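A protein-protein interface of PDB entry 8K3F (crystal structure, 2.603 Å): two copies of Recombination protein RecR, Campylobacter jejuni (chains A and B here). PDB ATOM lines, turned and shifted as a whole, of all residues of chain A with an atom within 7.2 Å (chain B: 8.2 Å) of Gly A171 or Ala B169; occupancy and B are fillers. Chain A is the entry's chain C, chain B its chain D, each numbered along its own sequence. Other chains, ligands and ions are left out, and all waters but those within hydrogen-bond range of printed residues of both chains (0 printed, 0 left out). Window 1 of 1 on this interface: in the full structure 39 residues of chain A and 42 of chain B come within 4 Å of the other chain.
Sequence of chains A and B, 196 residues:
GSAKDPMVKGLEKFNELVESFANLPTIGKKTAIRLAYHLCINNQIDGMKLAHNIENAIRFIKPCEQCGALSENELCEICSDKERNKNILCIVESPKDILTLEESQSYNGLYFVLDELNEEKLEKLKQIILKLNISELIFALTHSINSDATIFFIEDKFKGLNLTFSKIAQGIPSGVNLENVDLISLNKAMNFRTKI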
ATOM      1  N   HIS A 143     -24.589 -22.774 -16.324  1.00  0.00           N
ATOM      2  CA  HIS A 143     -23.628 -21.688 -16.507  1.00  0.00           C
ATOM      3  C   HIS A 143     -23.749 -20.710 -15.346  1.00  0.00           C
ATOM      4  O   HIS A 143     -24.753 -20.000 -15.222  1.00  0.00           O
ATOM      5  CB  HIS A 143     -23.860 -20.986 -17.840  1.00  0.00           C
ATOM      6  CG  HIS A 143     -23.838 -21.909 -19.017  1.00  0.00           C
ATOM      7  ND1 HIS A 143     -22.811 -22.800 -19.243  1.00  0.00           N
ATOM      8  CD2 HIS A 143     -24.717 -22.082 -20.034  1.00  0.00           C
ATOM      9  CE1 HIS A 143     -23.059 -23.483 -20.348  1.00  0.00           C
ATOM     10  NE2 HIS A 143     -24.208 -23.066 -20.848  1.00  0.00           N
ATOM     11  N   ILE A 168     -21.153 -27.565 -22.648  1.00  0.00           N
ATOM     12  CA  ILE A 168     -22.343 -27.411 -23.479  1.00  0.00           C
ATOM     13  C   ILE A 168     -22.511 -25.934 -23.800  1.00  0.00           C
ATOM     14  O   ILE A 168     -22.177 -25.065 -22.983  1.00  0.00           O
ATOM     15  CB  ILE A 168     -23.608 -27.962 -22.803  1.00  0.00           C
ATOM     16  CG1 ILE A 168     -23.866 -27.227 -21.490  1.00  0.00           C
ATOM     17  CG2 ILE A 168     -23.481 -29.460 -22.572  1.00  0.00           C
ATOM     18  CD1 ILE A 168     -24.934 -27.859 -20.666  1.00  0.00           C
ATOM     19  N   ALA A 169     -23.022 -25.651 -24.994  1.00  0.00           N
ATOM     20  CA  ALA A 169     -23.058 -24.285 -25.491  1.00  0.00           C
ATOM     21  C   ALA A 169     -23.862 -23.383 -24.562  1.00  0.00           C
ATOM     22  O   ALA A 169     -24.930 -23.757 -24.064  1.00  0.00           O
ATOM     23  CB  ALA A 169     -23.641 -24.254 -26.905  1.00  0.00           C
ATOM     24  N   GLN A 170     -23.311 -22.201 -24.301  1.00  0.00           N
ATOM     25  CA  GLN A 170     -24.022 -21.108 -23.660  1.00  0.00           C
ATOM     26  C   GLN A 170     -24.440 -20.135 -24.759  1.00  0.00           C
ATOM     27  O   GLN A 170     -23.590 -19.643 -25.507  1.00  0.00           O
ATOM     28  CB  GLN A 170     -23.141 -20.432 -22.608  1.00  0.00           C
ATOM     29  CG  GLN A 170     -23.784 -19.248 -21.905  1.00  0.00           C
ATOM     30  CD  GLN A 170     -23.017 -18.819 -20.667  1.00  0.00           C
ATOM     31  OE1 GLN A 170     -21.977 -19.389 -20.340  1.00  0.00           O
ATOM     32  NE2 GLN A 170     -23.532 -17.814 -19.969  1.00  0.00           N
ATOM     33  N   GLY A 171     -25.745 -19.893 -24.883  1.00  0.00           N
ATOM     34  CA  GLY A 171     -26.262 -19.106 -25.989  1.00  0.00           C
ATOM     35  C   GLY A 171     -27.753 -18.840 -25.914  1.00  0.00           C
ATOM     36  O   GLY A 171     -28.335 -18.829 -24.824  1.00  0.00           O
ATOM     37  N   ILE A 172     -28.383 -18.630 -27.067  1.00  0.00           N
ATOM     38  CA  ILE A 172     -29.777 -18.213 -27.142  1.00  0.00           C
ATOM     39  C   ILE A 172     -30.639 -19.465 -27.296  1.00  0.00           C
ATOM     40  O   ILE A 172     -30.429 -20.226 -28.253  1.00  0.00           O
ATOM     41  CB  ILE A 172     -30.014 -17.241 -28.306  1.00  0.00           C
ATOM     42  CG1 ILE A 172     -28.959 -16.142 -28.298  1.00  0.00           C
ATOM     43  CG2 ILE A 172     -31.400 -16.614 -28.224  1.00  0.00           C
ATOM     44  CD1 ILE A 172     -28.845 -15.436 -26.973  1.00  0.00           C
ATOM     45  N   PRO A 173     -31.608 -19.698 -26.424  1.00  0.00           N
ATOM     46  CA  PRO A 173     -32.443 -20.896 -26.555  1.00  0.00           C
ATOM     47  C   PRO A 173     -33.433 -20.756 -27.701  1.00  0.00           C
ATOM     48  O   PRO A 173     -33.659 -19.676 -28.252  1.00  0.00           O
ATOM     49  CB  PRO A 173     -33.170 -20.989 -25.209  1.00  0.00           C
ATOM     50  CG  PRO A 173     -32.681 -19.822 -24.393  1.00  0.00           C
ATOM     51  CD  PRO A 173     -32.050 -18.839 -25.319  1.00  0.00           C
ATOM     52  N   VAL A 181     -32.622 -12.712 -23.106  1.00  0.00           N
ATOM     53  CA  VAL A 181     -31.501 -13.471 -22.584  1.00  0.00           C
ATOM     54  C   VAL A 181     -30.571 -12.512 -21.853  1.00  0.00           C
ATOM     55  O   VAL A 181     -30.603 -11.294 -22.054  1.00  0.00           O
ATOM     56  CB  VAL A 181     -30.760 -14.239 -23.697  1.00  0.00           C
ATOM     57  CG1 VAL A 181     -30.739 -15.723 -23.385  1.00  0.00           C
ATOM     58  CG2 VAL A 181     -31.439 -13.995 -25.035  1.00  0.00           C
ATOM     59  N   ASP A 182     -29.744 -13.074 -20.976  1.00  0.00           N
ATOM     60  CA  ASP A 182     -28.788 -12.266 -20.235  1.00  0.00           C
ATOM     61  C   ASP A 182     -27.645 -11.835 -21.144  1.00  0.00           C
ATOM     62  O   ASP A 182     -27.281 -12.531 -22.095  1.00  0.00           O
ATOM     63  CB  ASP A 182     -28.249 -13.033 -19.029  1.00  0.00           C
ATOM     64  CG  ASP A 182     -27.859 -14.455 -19.371  1.00  0.00           C
ATOM     65  OD1 ASP A 182     -26.666 -14.704 -19.640  1.00  0.00           O
ATOM     66  OD2 ASP A 182     -28.752 -15.327 -19.377  1.00  0.00           O
ATOM     67  N   ILE A 184     -24.511 -11.737 -20.847  1.00  0.00           N
ATOM     68  CA  ILE A 184     -23.326 -12.589 -20.921  1.00  0.00           C
ATOM     69  C   ILE A 184     -23.538 -13.708 -21.932  1.00  0.00           C
ATOM     70  O   ILE A 184     -22.664 -13.986 -22.761  1.00  0.00           O
ATOM     71  CB  ILE A 184     -22.972 -13.147 -19.528  1.00  0.00           C
ATOM     72  CG1 ILE A 184     -22.702 -12.007 -18.543  1.00  0.00           C
ATOM     73  CG2 ILE A 184     -21.766 -14.078 -19.613  1.00  0.00           C
ATOM     74  CD1 ILE A 184     -22.328 -12.471 -17.146  1.00  0.00           C
ATOM     75  N   SER A 185     -24.699 -14.368 -21.877  1.00  0.00           N
ATOM     76  CA  SER A 185     -25.000 -15.424 -22.842  1.00  0.00           C
ATOM     77  C   SER A 185     -25.078 -14.865 -24.255  1.00  0.00           C
ATOM     78  O   SER A 185     -24.652 -15.515 -25.217  1.00  0.00           O
ATOM     79  CB  SER A 185     -26.312 -16.123 -22.475  1.00  0.00           C
ATOM     80  OG  SER A 185     -26.261 -16.646 -21.161  1.00  0.00           O
ATOM     81  N   LEU A 186     -25.629 -13.661 -24.394  1.00  0.00           N
ATOM     82  CA  LEU A 186     -25.650 -12.976 -25.680  1.00  0.00           C
ATOM     83  C   LEU A 186     -24.231 -12.696 -26.169  1.00  0.00           C
ATOM     84  O   LEU A 186     -23.877 -13.021 -27.310  1.00  0.00           O
ATOM     85  CB  LEU A 186     -26.451 -11.683 -25.530  1.00  0.00           C
ATOM     86  CG  LEU A 186     -27.169 -11.079 -26.724  1.00  0.00           C
ATOM     87  CD1 LEU A 186     -27.794 -12.162 -27.572  1.00  0.00           C
ATOM     88  CD2 LEU A 186     -28.228 -10.145 -26.196  1.00  0.00           C
ATOM     89  N   LYS A 188     -21.547 -14.241 -25.411  1.00  0.00           N
ATOM     90  CA  LYS A 188     -20.930 -15.498 -25.820  1.00  0.00           C
ATOM     91  C   LYS A 188     -21.575 -16.069 -27.075  1.00  0.00           C
ATOM     92  O   LYS A 188     -20.882 -16.675 -27.902  1.00  0.00           O
ATOM     93  CB  LYS A 188     -20.999 -16.510 -24.677  1.00  0.00           C
ATOM     94  CG  LYS A 188     -19.981 -16.261 -23.584  1.00  0.00           C
ATOM     95  CD  LYS A 188     -20.431 -16.871 -22.276  1.00  0.00           C
ATOM     96  CE  LYS A 188     -19.262 -17.093 -21.346  1.00  0.00           C
ATOM     97  NZ  LYS A 188     -19.745 -17.377 -19.973  1.00  0.00           N
ATOM     98  N   ALA A 189     -22.890 -15.891 -27.239  1.00  0.00           N
ATOM     99  CA  ALA A 189     -23.545 -16.377 -28.448  1.00  0.00           C
ATOM    100  C   ALA A 189     -23.011 -15.678 -29.690  1.00  0.00           C
ATOM    101  O   ALA A 189     -22.999 -16.268 -30.775  1.00  0.00           O
ATOM    102  CB  ALA A 189     -25.059 -16.195 -28.342  1.00  0.00           C
ATOM    103  N   MET A 190     -22.552 -14.433 -29.554  1.00  0.00           N
ATOM    104  CA  MET A 190     -21.966 -13.707 -30.673  1.00  0.00           C
ATOM    105  C   MET A 190     -20.473 -13.962 -30.846  1.00  0.00           C
ATOM    106  O   MET A 190     -19.954 -13.788 -31.953  1.00  0.00           O
ATOM    107  CB  MET A 190     -22.205 -12.203 -30.505  1.00  0.00           C
ATOM    108  CG  MET A 190     -23.379 -11.667 -31.309  1.00  0.00           C
ATOM    109  SD  MET A 190     -23.010 -11.584 -33.076  1.00  0.00           S
ATOM    110  CE  MET A 190     -23.463  -9.889 -33.437  1.00  0.00           C
ATOM    111  N   ASN A 191     -19.770 -14.359 -29.783  1.00  0.00           N
ATOM    112  CA  ASN A 191     -18.341 -14.630 -29.858  1.00  0.00           C
ATOM    113  C   ASN A 191     -18.023 -16.059 -30.272  1.00  0.00           C
ATOM    114  O   ASN A 191     -16.872 -16.349 -30.604  1.00  0.00           O
ATOM    115  CB  ASN A 191     -17.669 -14.338 -28.507  1.00  0.00           C
ATOM    116  CG  ASN A 191     -17.429 -12.856 -28.281  1.00  0.00           C
ATOM    117  OD1 ASN A 191     -16.967 -12.144 -29.175  1.00  0.00           O
ATOM    118  ND2 ASN A 191     -17.742 -12.383 -27.081  1.00  0.00           N
ATOM    119  N   PHE A 192     -19.002 -16.958 -30.259  1.00  0.00           N
ATOM    120  CA  PHE A 192     -18.783 -18.359 -30.606  1.00  0.00           C
ATOM    121  C   PHE A 192     -19.871 -18.811 -31.581  1.00  0.00           C
ATOM    122  O   PHE A 192     -20.639 -19.732 -31.317  1.00  0.00           O
ATOM    123  CB  PHE A 192     -18.737 -19.221 -29.342  1.00  0.00           C
ATOM    124  CG  PHE A 192     -17.564 -18.915 -28.451  1.00  0.00           C
ATOM    125  CD1 PHE A 192     -16.392 -19.651 -28.546  1.00  0.00           C
ATOM    126  CD2 PHE A 192     -17.623 -17.876 -27.532  1.00  0.00           C
ATOM    127  CE1 PHE A 192     -15.306 -19.362 -27.738  1.00  0.00           C
ATOM    128  CE2 PHE A 192     -16.537 -17.581 -26.724  1.00  0.00           C
ATOM    129  CZ  PHE A 192     -15.380 -18.326 -26.827  1.00  0.00           C
ATOM    130  N   ARG A 193     -19.920 -18.149 -32.734  1.00  0.00           N
ATOM    131  CA  ARG A 193     -20.968 -18.400 -33.711  1.00  0.00           C
ATOM    132  C   ARG A 193     -20.731 -19.716 -34.443  1.00  0.00           C
ATOM    133  O   ARG A 193     -19.602 -20.200 -34.548  1.00  0.00           O
ATOM    134  CB  ARG A 193     -21.027 -17.251 -34.713  1.00  0.00           C
ATOM    135  CG  ARG A 193     -20.771 -15.905 -34.078  1.00  0.00           C
ATOM    136  CD  ARG A 193     -20.893 -14.777 -35.084  1.00  0.00           C
ATOM    137  NE  ARG A 193     -19.769 -14.707 -36.011  1.00  0.00           N
ATOM    138  CZ  ARG A 193     -18.740 -13.876 -35.876  1.00  0.00           C
ATOM    139  NH1 ARG A 193     -17.767 -13.868 -36.776  1.00  0.00           N
ATOM    140  NH2 ARG A 193     -18.687 -13.048 -34.842  1.00  0.00           N
ATOM    141  N   THR A 194     -21.813 -20.296 -34.953  1.00  0.00           N
ATOM    142  CA  THR A 194     -21.756 -21.533 -35.715  1.00  0.00           C
ATOM    143  C   THR A 194     -21.959 -21.228 -37.198  1.00  0.00           C
ATOM    144  O   THR A 194     -21.832 -20.085 -37.641  1.00  0.00           O
ATOM    145  CB  THR A 194     -22.793 -22.538 -35.201  1.00  0.00           C
ATOM    146  OG1 THR A 194     -24.081 -22.232 -35.755  1.00  0.00           O
ATOM    147  CG2 THR A 194     -22.870 -22.498 -33.679  1.00  0.00           C
ATOM    148  N   ILE B 138     -23.439 -12.322 -40.528  1.00  0.00           N
ATOM    149  CA  ILE B 138     -23.790 -12.896 -39.232  1.00  0.00           C
ATOM    150  C   ILE B 138     -25.303 -12.835 -39.083  1.00  0.00           C
ATOM    151  O   ILE B 138     -25.881 -11.743 -39.034  1.00  0.00           O
ATOM    152  CB  ILE B 138     -23.109 -12.150 -38.073  1.00  0.00           C
ATOM    153  CG1 ILE B 138     -21.583 -12.194 -38.195  1.00  0.00           C
ATOM    154  CG2 ILE B 138     -23.556 -12.731 -36.744  1.00  0.00           C
ATOM    155  CD1 ILE B 138     -20.880 -11.439 -37.091  1.00  0.00           C
ATOM    156  N   PHE B 139     -25.946 -13.999 -38.996  1.00  0.00           N
ATOM    157  CA  PHE B 139     -27.389 -14.081 -38.756  1.00  0.00           C
ATOM    158  C   PHE B 139     -27.636 -14.042 -37.249  1.00  0.00           C
ATOM    159  O   PHE B 139     -27.462 -15.046 -36.552  1.00  0.00           O
ATOM    160  CB  PHE B 139     -27.976 -15.350 -39.374  1.00  0.00           C
ATOM    161  CG  PHE B 139     -27.900 -15.398 -40.879  1.00  0.00           C
ATOM    162  CD1 PHE B 139     -28.861 -14.765 -41.656  1.00  0.00           C
ATOM    163  CD2 PHE B 139     -26.877 -16.090 -41.515  1.00  0.00           C
ATOM    164  CE1 PHE B 139     -28.800 -14.811 -43.034  1.00  0.00           C
ATOM    165  CE2 PHE B 139     -26.810 -16.145 -42.892  1.00  0.00           C
ATOM    166  CZ  PHE B 139     -27.773 -15.503 -43.655  1.00  0.00           C
ATOM    167  N   ALA B 140     -28.041 -12.885 -36.735  1.00  0.00           N
ATOM    168  CA  ALA B 140     -28.404 -12.763 -35.321  1.00  0.00           C
ATOM    169  C   ALA B 140     -29.918 -12.866 -35.149  1.00  0.00           C
ATOM    170  O   ALA B 140     -30.581 -11.974 -34.626  1.00  0.00           O
ATOM    171  CB  ALA B 140     -27.867 -11.459 -34.740  1.00  0.00           C
ATOM    172  N   LEU B 141     -30.464 -13.980 -35.617  1.00  0.00           N
ATOM    173  CA  LEU B 141     -31.895 -14.230 -35.568  1.00  0.00           C
ATOM    174  C   LEU B 141     -32.233 -15.110 -34.374  1.00  0.00           C
ATOM    175  O   LEU B 141     -31.404 -15.891 -33.898  1.00  0.00           O
ATOM    176  CB  LEU B 141     -32.384 -14.901 -36.856  1.00  0.00           C
ATOM    177  CG  LEU B 141     -31.999 -14.201 -38.158  1.00  0.00           C
ATOM    178  CD1 LEU B 141     -32.612 -14.902 -39.359  1.00  0.00           C
ATOM    179  CD2 LEU B 141     -32.408 -12.735 -38.112  1.00  0.00           C
ATOM    180  N   HIS B 143     -33.740 -18.327 -32.696  1.00  0.00           N
ATOM    181  CA  HIS B 143     -33.706 -19.699 -33.180  1.00  0.00           C
ATOM    182  C   HIS B 143     -35.144 -20.197 -33.270  1.00  0.00           C
ATOM    183  O   HIS B 143     -35.786 -20.461 -32.249  1.00  0.00           O
ATOM    184  CB  HIS B 143     -32.821 -20.554 -32.282  1.00  0.00           C
ATOM    185  CG  HIS B 143     -31.393 -20.113 -32.292  1.00  0.00           C
ATOM    186  ND1 HIS B 143     -30.625 -20.121 -33.439  1.00  0.00           N
ATOM    187  CD2 HIS B 143     -30.605 -19.603 -31.317  1.00  0.00           C
ATOM    188  CE1 HIS B 143     -29.419 -19.657 -33.163  1.00  0.00           C
ATOM    189  NE2 HIS B 143     -29.381 -19.335 -31.882  1.00  0.00           N
ATOM    190  N   SER B 166     -22.531 -17.177 -40.918  1.00  0.00           N
ATOM    191  CA  SER B 166     -22.519 -17.672 -39.548  1.00  0.00           C
ATOM    192  C   SER B 166     -23.772 -17.190 -38.831  1.00  0.00           C
ATOM    193  O   SER B 166     -24.428 -16.233 -39.257  1.00  0.00           O
ATOM    194  CB  SER B 166     -21.261 -17.222 -38.784  1.00  0.00           C
ATOM    195  OG  SER B 166     -21.271 -15.826 -38.543  1.00  0.00           O
ATOM    196  N   LYS B 167     -24.105 -17.868 -37.733  1.00  0.00           N
ATOM    197  CA  LYS B 167     -25.256 -17.483 -36.925  1.00  0.00           C
ATOM    198  C   LYS B 167     -24.874 -17.539 -35.455  1.00  0.00           C
ATOM    199  O   LYS B 167     -24.005 -18.322 -35.058  1.00  0.00           O
ATOM    200  CB  LYS B 167     -26.478 -18.381 -37.198  1.00  0.00           C
ATOM    201  CG  LYS B 167     -26.292 -19.834 -36.830  1.00  0.00           C
ATOM    202  CD  LYS B 167     -27.321 -20.700 -37.512  1.00  0.00           C
ATOM    203  CE  LYS B 167     -27.659 -21.880 -36.643  1.00  0.00           C
ATOM    204  NZ  LYS B 167     -28.316 -22.970 -37.408  1.00  0.00           N
ATOM    205  N   ILE B 168     -25.515 -16.682 -34.654  1.00  0.00           N
ATOM    206  CA  ILE B 168     -25.219 -16.663 -33.229  1.00  0.00           C
ATOM    207  C   ILE B 168     -25.569 -18.020 -32.639  1.00  0.00           C
ATOM    208  O   ILE B 168     -26.463 -18.727 -33.124  1.00  0.00           O
ATOM    209  CB  ILE B 168     -25.960 -15.535 -32.490  1.00  0.00           C
ATOM    210  CG1 ILE B 168     -27.473 -15.720 -32.602  1.00  0.00           C
ATOM    211  CG2 ILE B 168     -25.522 -14.177 -33.022  1.00  0.00           C
ATOM    212  CD1 ILE B 168     -28.261 -14.615 -31.951  1.00  0.00           C
ATOM    213  N   ALA B 169     -24.848 -18.390 -31.588  1.00  0.00           N
ATOM    214  CA  ALA B 169     -24.910 -19.747 -31.078  1.00  0.00           C
ATOM    215  C   ALA B 169     -26.245 -20.019 -30.400  1.00  0.00           C
ATOM    216  O   ALA B 169     -26.814 -19.152 -29.731  1.00  0.00           O
ATOM    217  CB  ALA B 169     -23.766 -19.991 -30.099  1.00  0.00           C
ATOM    218  N   GLN B 170     -26.748 -21.231 -30.591  1.00  0.00           N
ATOM    219  CA  GLN B 170     -27.902 -21.720 -29.859  1.00  0.00           C
ATOM    220  C   GLN B 170     -27.407 -22.536 -28.675  1.00  0.00           C
ATOM    221  O   GLN B 170     -26.459 -23.320 -28.798  1.00  0.00           O
ATOM    222  CB  GLN B 170     -28.811 -22.564 -30.758  1.00  0.00           C
ATOM    223  CG  GLN B 170     -30.170 -22.887 -30.149  1.00  0.00           C
ATOM    224  CD  GLN B 170     -31.140 -23.473 -31.162  1.00  0.00           C
ATOM    225  OE1 GLN B 170     -32.315 -23.701 -30.860  1.00  0.00           O
ATOM    226  NE2 GLN B 170     -30.650 -23.716 -32.377  1.00  0.00           N
ATOM    227  N   GLY B 171     -28.034 -22.330 -27.521  1.00  0.00           N
ATOM    228  CA  GLY B 171     -27.598 -23.010 -26.323  1.00  0.00           C
ATOM    229  C   GLY B 171     -28.415 -22.634 -25.111  1.00  0.00           C
ATOM    230  O   GLY B 171     -29.602 -22.319 -25.222  1.00  0.00           O
ATOM    231  N   ILE B 172     -27.778 -22.644 -23.947  1.00  0.00           N
ATOM    232  CA  ILE B 172     -28.466 -22.446 -22.676  1.00  0.00           C
ATOM    233  C   ILE B 172     -28.028 -21.112 -22.080  1.00  0.00           C
ATOM    234  O   ILE B 172     -26.830 -20.794 -22.093  1.00  0.00           O
ATOM    235  CB  ILE B 172     -28.182 -23.614 -21.720  1.00  0.00           C
ATOM    236  CG1 ILE B 172     -28.566 -24.937 -22.386  1.00  0.00           C
ATOM    237  CG2 ILE B 172     -28.916 -23.441 -20.399  1.00  0.00           C
ATOM    238  CD1 ILE B 172     -28.205 -26.145 -21.567  1.00  0.00           C
ATOM    239  N   PRO B 173     -28.943 -20.304 -21.559  1.00  0.00           N
ATOM    240  CA  PRO B 173     -28.558 -19.036 -20.937  1.00  0.00           C
ATOM    241  C   PRO B 173     -27.962 -19.273 -19.553  1.00  0.00           C
ATOM    242  O   PRO B 173     -27.872 -20.397 -19.068  1.00  0.00           O
ATOM    243  CB  PRO B 173     -29.881 -18.264 -20.839  1.00  0.00           C
ATOM    244  CG  PRO B 173     -30.904 -19.104 -21.529  1.00  0.00           C
ATOM    245  CD  PRO B 173     -30.399 -20.496 -21.555  1.00  0.00           C
ATOM    246  N   SER B 174     -27.580 -18.174 -18.912  1.00  0.00           N
ATOM    247  CA  SER B 174     -27.041 -18.225 -17.562  1.00  0.00           C
ATOM    248  C   SER B 174     -28.106 -18.641 -16.551  1.00  0.00           C
ATOM    249  O   SER B 174     -29.287 -18.313 -16.685  1.00  0.00           O
ATOM    250  CB  SER B 174     -26.472 -16.860 -17.164  1.00  0.00           C
ATOM    251  OG  SER B 174     -25.283 -16.576 -17.878  1.00  0.00           O
ATOM    252  N   VAL B 176     -29.739 -21.247 -15.698  1.00  0.00           N
ATOM    253  CA  VAL B 176     -30.899 -22.053 -16.057  1.00  0.00           C
ATOM    254  C   VAL B 176     -30.552 -23.519 -15.847  1.00  0.00           C
ATOM    255  O   VAL B 176     -29.500 -23.982 -16.300  1.00  0.00           O
ATOM    256  CB  VAL B 176     -31.333 -21.789 -17.508  1.00  0.00           C
ATOM    257  CG1 VAL B 176     -32.580 -22.580 -17.837  1.00  0.00           C
ATOM    258  CG2 VAL B 176     -31.564 -20.298 -17.726  1.00  0.00           C
ATOM    259  N   SER B 185     -33.148 -27.182 -27.758  1.00  0.00           N
ATOM    260  CA  SER B 185     -32.007 -26.338 -27.410  1.00  0.00           C
ATOM    261  C   SER B 185     -30.942 -27.137 -26.678  1.00  0.00           C
ATOM    262  O   SER B 185     -29.743 -26.900 -26.862  1.00  0.00           O
ATOM    263  CB  SER B 185     -32.449 -25.150 -26.561  1.00  0.00           C
ATOM    264  OG  SER B 185     -32.977 -24.121 -27.373  1.00  0.00           O
ATOM    265  N   LYS B 188     -28.989 -29.030 -29.295  1.00  0.00           N
ATOM    266  CA  LYS B 188     -28.051 -28.157 -29.992  1.00  0.00           C
ATOM    267  C   LYS B 188     -26.905 -27.742 -29.081  1.00  0.00           C
ATOM    268  O   LYS B 188     -25.756 -27.663 -29.526  1.00  0.00           O
ATOM    269  CB  LYS B 188     -28.775 -26.927 -30.538  1.00  0.00           C
ATOM    270  CG  LYS B 188     -29.845 -27.230 -31.586  1.00  0.00           C
ATOM    271  CD  LYS B 188     -29.243 -27.425 -32.967  1.00  0.00           C
ATOM    272  CE  LYS B 188     -29.945 -26.555 -34.003  1.00  0.00           C
ATOM    273  NZ  LYS B 188     -29.089 -26.319 -35.201  1.00  0.00           N
ATOM    274  N   ALA B 189     -27.194 -27.479 -27.803  1.00  0.00           N
ATOM    275  CA  ALA B 189     -26.133 -27.102 -26.869  1.00  0.00           C
ATOM    276  C   ALA B 189     -25.130 -28.230 -26.657  1.00  0.00           C
ATOM    277  O   ALA B 189     -23.953 -27.970 -26.391  1.00  0.00           O
ATOM    278  CB  ALA B 189     -26.728 -26.676 -25.525  1.00  0.00           C
ATOM    279  N   PHE B 192     -23.175 -28.940 -30.200  1.00  0.00           N
ATOM    280  CA  PHE B 192     -22.304 -27.824 -30.543  1.00  0.00           C
ATOM    281  C   PHE B 192     -21.625 -27.265 -29.303  1.00  0.00           C
ATOM    282  O   PHE B 192     -21.423 -26.054 -29.168  1.00  0.00           O
ATOM    283  CB  PHE B 192     -23.082 -26.745 -31.290  1.00  0.00           C
ATOM    284  CG  PHE B 192     -23.652 -27.224 -32.594  1.00  0.00           C
ATOM    285  CD1 PHE B 192     -22.889 -27.190 -33.751  1.00  0.00           C
ATOM    286  CD2 PHE B 192     -24.938 -27.737 -32.658  1.00  0.00           C
ATOM    287  CE1 PHE B 192     -23.403 -27.645 -34.948  1.00  0.00           C
ATOM    288  CE2 PHE B 192     -25.459 -28.192 -33.854  1.00  0.00           C
ATOM    289  CZ  PHE B 192     -24.689 -28.147 -35.000  1.00  0.00           C
ATOM    290  N   THR B 194     -18.731 -26.176 -26.782  1.00  0.00           N
ATOM    291  CA  THR B 194     -17.561 -25.370 -27.088  1.00  0.00           C
ATOM    292  C   THR B 194     -16.392 -25.778 -26.203  1.00  0.00           C
ATOM    293  O   THR B 194     -16.572 -26.208 -25.066  1.00  0.00           O
ATOM    294  CB  THR B 194     -17.859 -23.871 -26.924  1.00  0.00           C
ATOM    295  OG1 THR B 194     -17.609 -23.469 -25.574  1.00  0.00           O
ATOM    296  CG2 THR B 194     -19.318 -23.574 -27.281  1.00  0.00           C
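O of Ile A172 lies within hydrogen-bond range of N of Gly B171, 3.3 Å away.
The side-chain hydroxyl (OG) of Ser B174 sits at hydrogen-bond distance from the side-chain carboxylate (OD1) of Asp A182, at 2.9 Å.
The backbone NH of Gly A171 sits at hydrogen-bond distance from the backbone carbonyl oxygen of Ile B172.
The backbone carbonyl oxygen (O) of Ala A169 lies within hydrogen-bond range of the backbone NH (N) of Ile B172, 3.1 Å away.
OG of Ser B174 sits at hydrogen-bond distance from NE2 of Gln A170, 3.0 Å away.
OG of Ser A185 is in hydrogen-bond range of N of Ser B174.
The backbone carbonyl oxygen (O) of Ala B169 sits at hydrogen-bond distance from the backbone NH (N) of Ile A172.
O of Ala A189 sits at hydrogen-bond distance from N of Ala B169.
O of Ala B189 is in hydrogen-bond range of N of Ala A169, at 2.9 Å.
The guanidinium group (NE) of Arg A193 is in hydrogen-bond range of the side-chain hydroxyl (OG) of Ser B166 (3.1 Å).
The backbone NH (N) of Thr A194 is in hydrogen-bond range of the backbone carbonyl oxygen (O) of Lys B167 (3.0 Å).
NE2 of His A143 is in hydrogen-bond range of O of Ala A169, at 3.4 Å.
OE1 of Gln A170 lies within hydrogen-bond range of NZ of Lys A188, 3.0 Å away.
O of Ile B168 lies close to NE2 of His B143, 3.2 Å away.
The backbone carbonyl oxygen of Ser B166 lies within hydrogen-bond range of the backbone NH of Phe B139.
OD1 of Asp A182 is in hydrogen-bond range of OG of Ser A185.
NE2 of His B143 lies close to N of Gln B170 (3.5 Å).
Among the printed residues, merely in contact across the chains: His A143 with Ile B172, His A143 with Pro B173, His A143 with Ser B174, Ile A168 with Ile B172, Ile A168 with Ala B189, Ala A169 with Gln B170, Ala A169 with Gly B171, Ala A169 with Phe B192, Gln A170 with Ile B172, Gly A171 with Ala B169, Gly A171 with Gly B171, Gly A171 with Pro B173, Ile A172 with His B143, Ile A172 with Gln B170, Pro A173 with Gly B171, Pro A173 with Pro B173, Pro A173 with Ser B185, Val A181 with Pro B173, Asp A182 with Pro B173, Ser A185 with Pro B173, Ala A189 with Ile B168, Met A190 with Ile B138, Met A190 with Ile B168, Phe A192 with Ala B169, Arg A193 with Ile B138, Arg A193 with Lys B167 and Thr A194 with Ser B166.
Of the printed residues of chain B, Ala A169 touches Gln B170 (3.5 Å), Gly B171 (3.6 Å), Ile B172 (3.1 Å), Ala B189 (2.9 Å) and Phe B192 (3.6 Å).
Printed residues of chain B within 4 Å of Gly A171: Ala B169, Gly B171, Ile B172 and Pro B173.
Printed residues of chain B within 4 Å of Ile A172: His B143 (3.1 Å), Ala B169 (3.1 Å), Gln B170 (3.3 Å) and Gly B171 (3.3 Å).
Printed residues of chain B within 4 Å of Thr A194: Ser B166 and Lys B167.
Of chain A, only Gly A171, Ile A172, Ala A189 and Phe A192 come within 4 Å of Ala B169.
The nearest residue of chain B that does not touch Gly A171 is Gln B170 (4.5 Å).
The nearest residue of chain A that does not touch Ala B169 is Thr A194 (4.3 Å).
The nearest printed residue of chain B that does not touch Phe A192 is Thr B194 (4.8 Å).
Among the printed residues, 38 pairs touch across the chains.
Among the printed residues, no Asp or Glu carboxylate lies within 4 Å of a Lys or Arg side-chain nitrogen of the other chain.
His A143 touches Pro B173, but with the chains exchanged Pro A173 does not touch His B143 (4.2 Å).
Ala A169 touches Ile B172, and with the chains exchanged Ile A172 touches Ala B169.
Ala A169 touches Ala B189, and with the chains exchanged Ala A189 touches Ala B169.
Of the 38 pairs that touch across the chains among the printed residues, 22 have their exchanged pair printed and touching as well.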
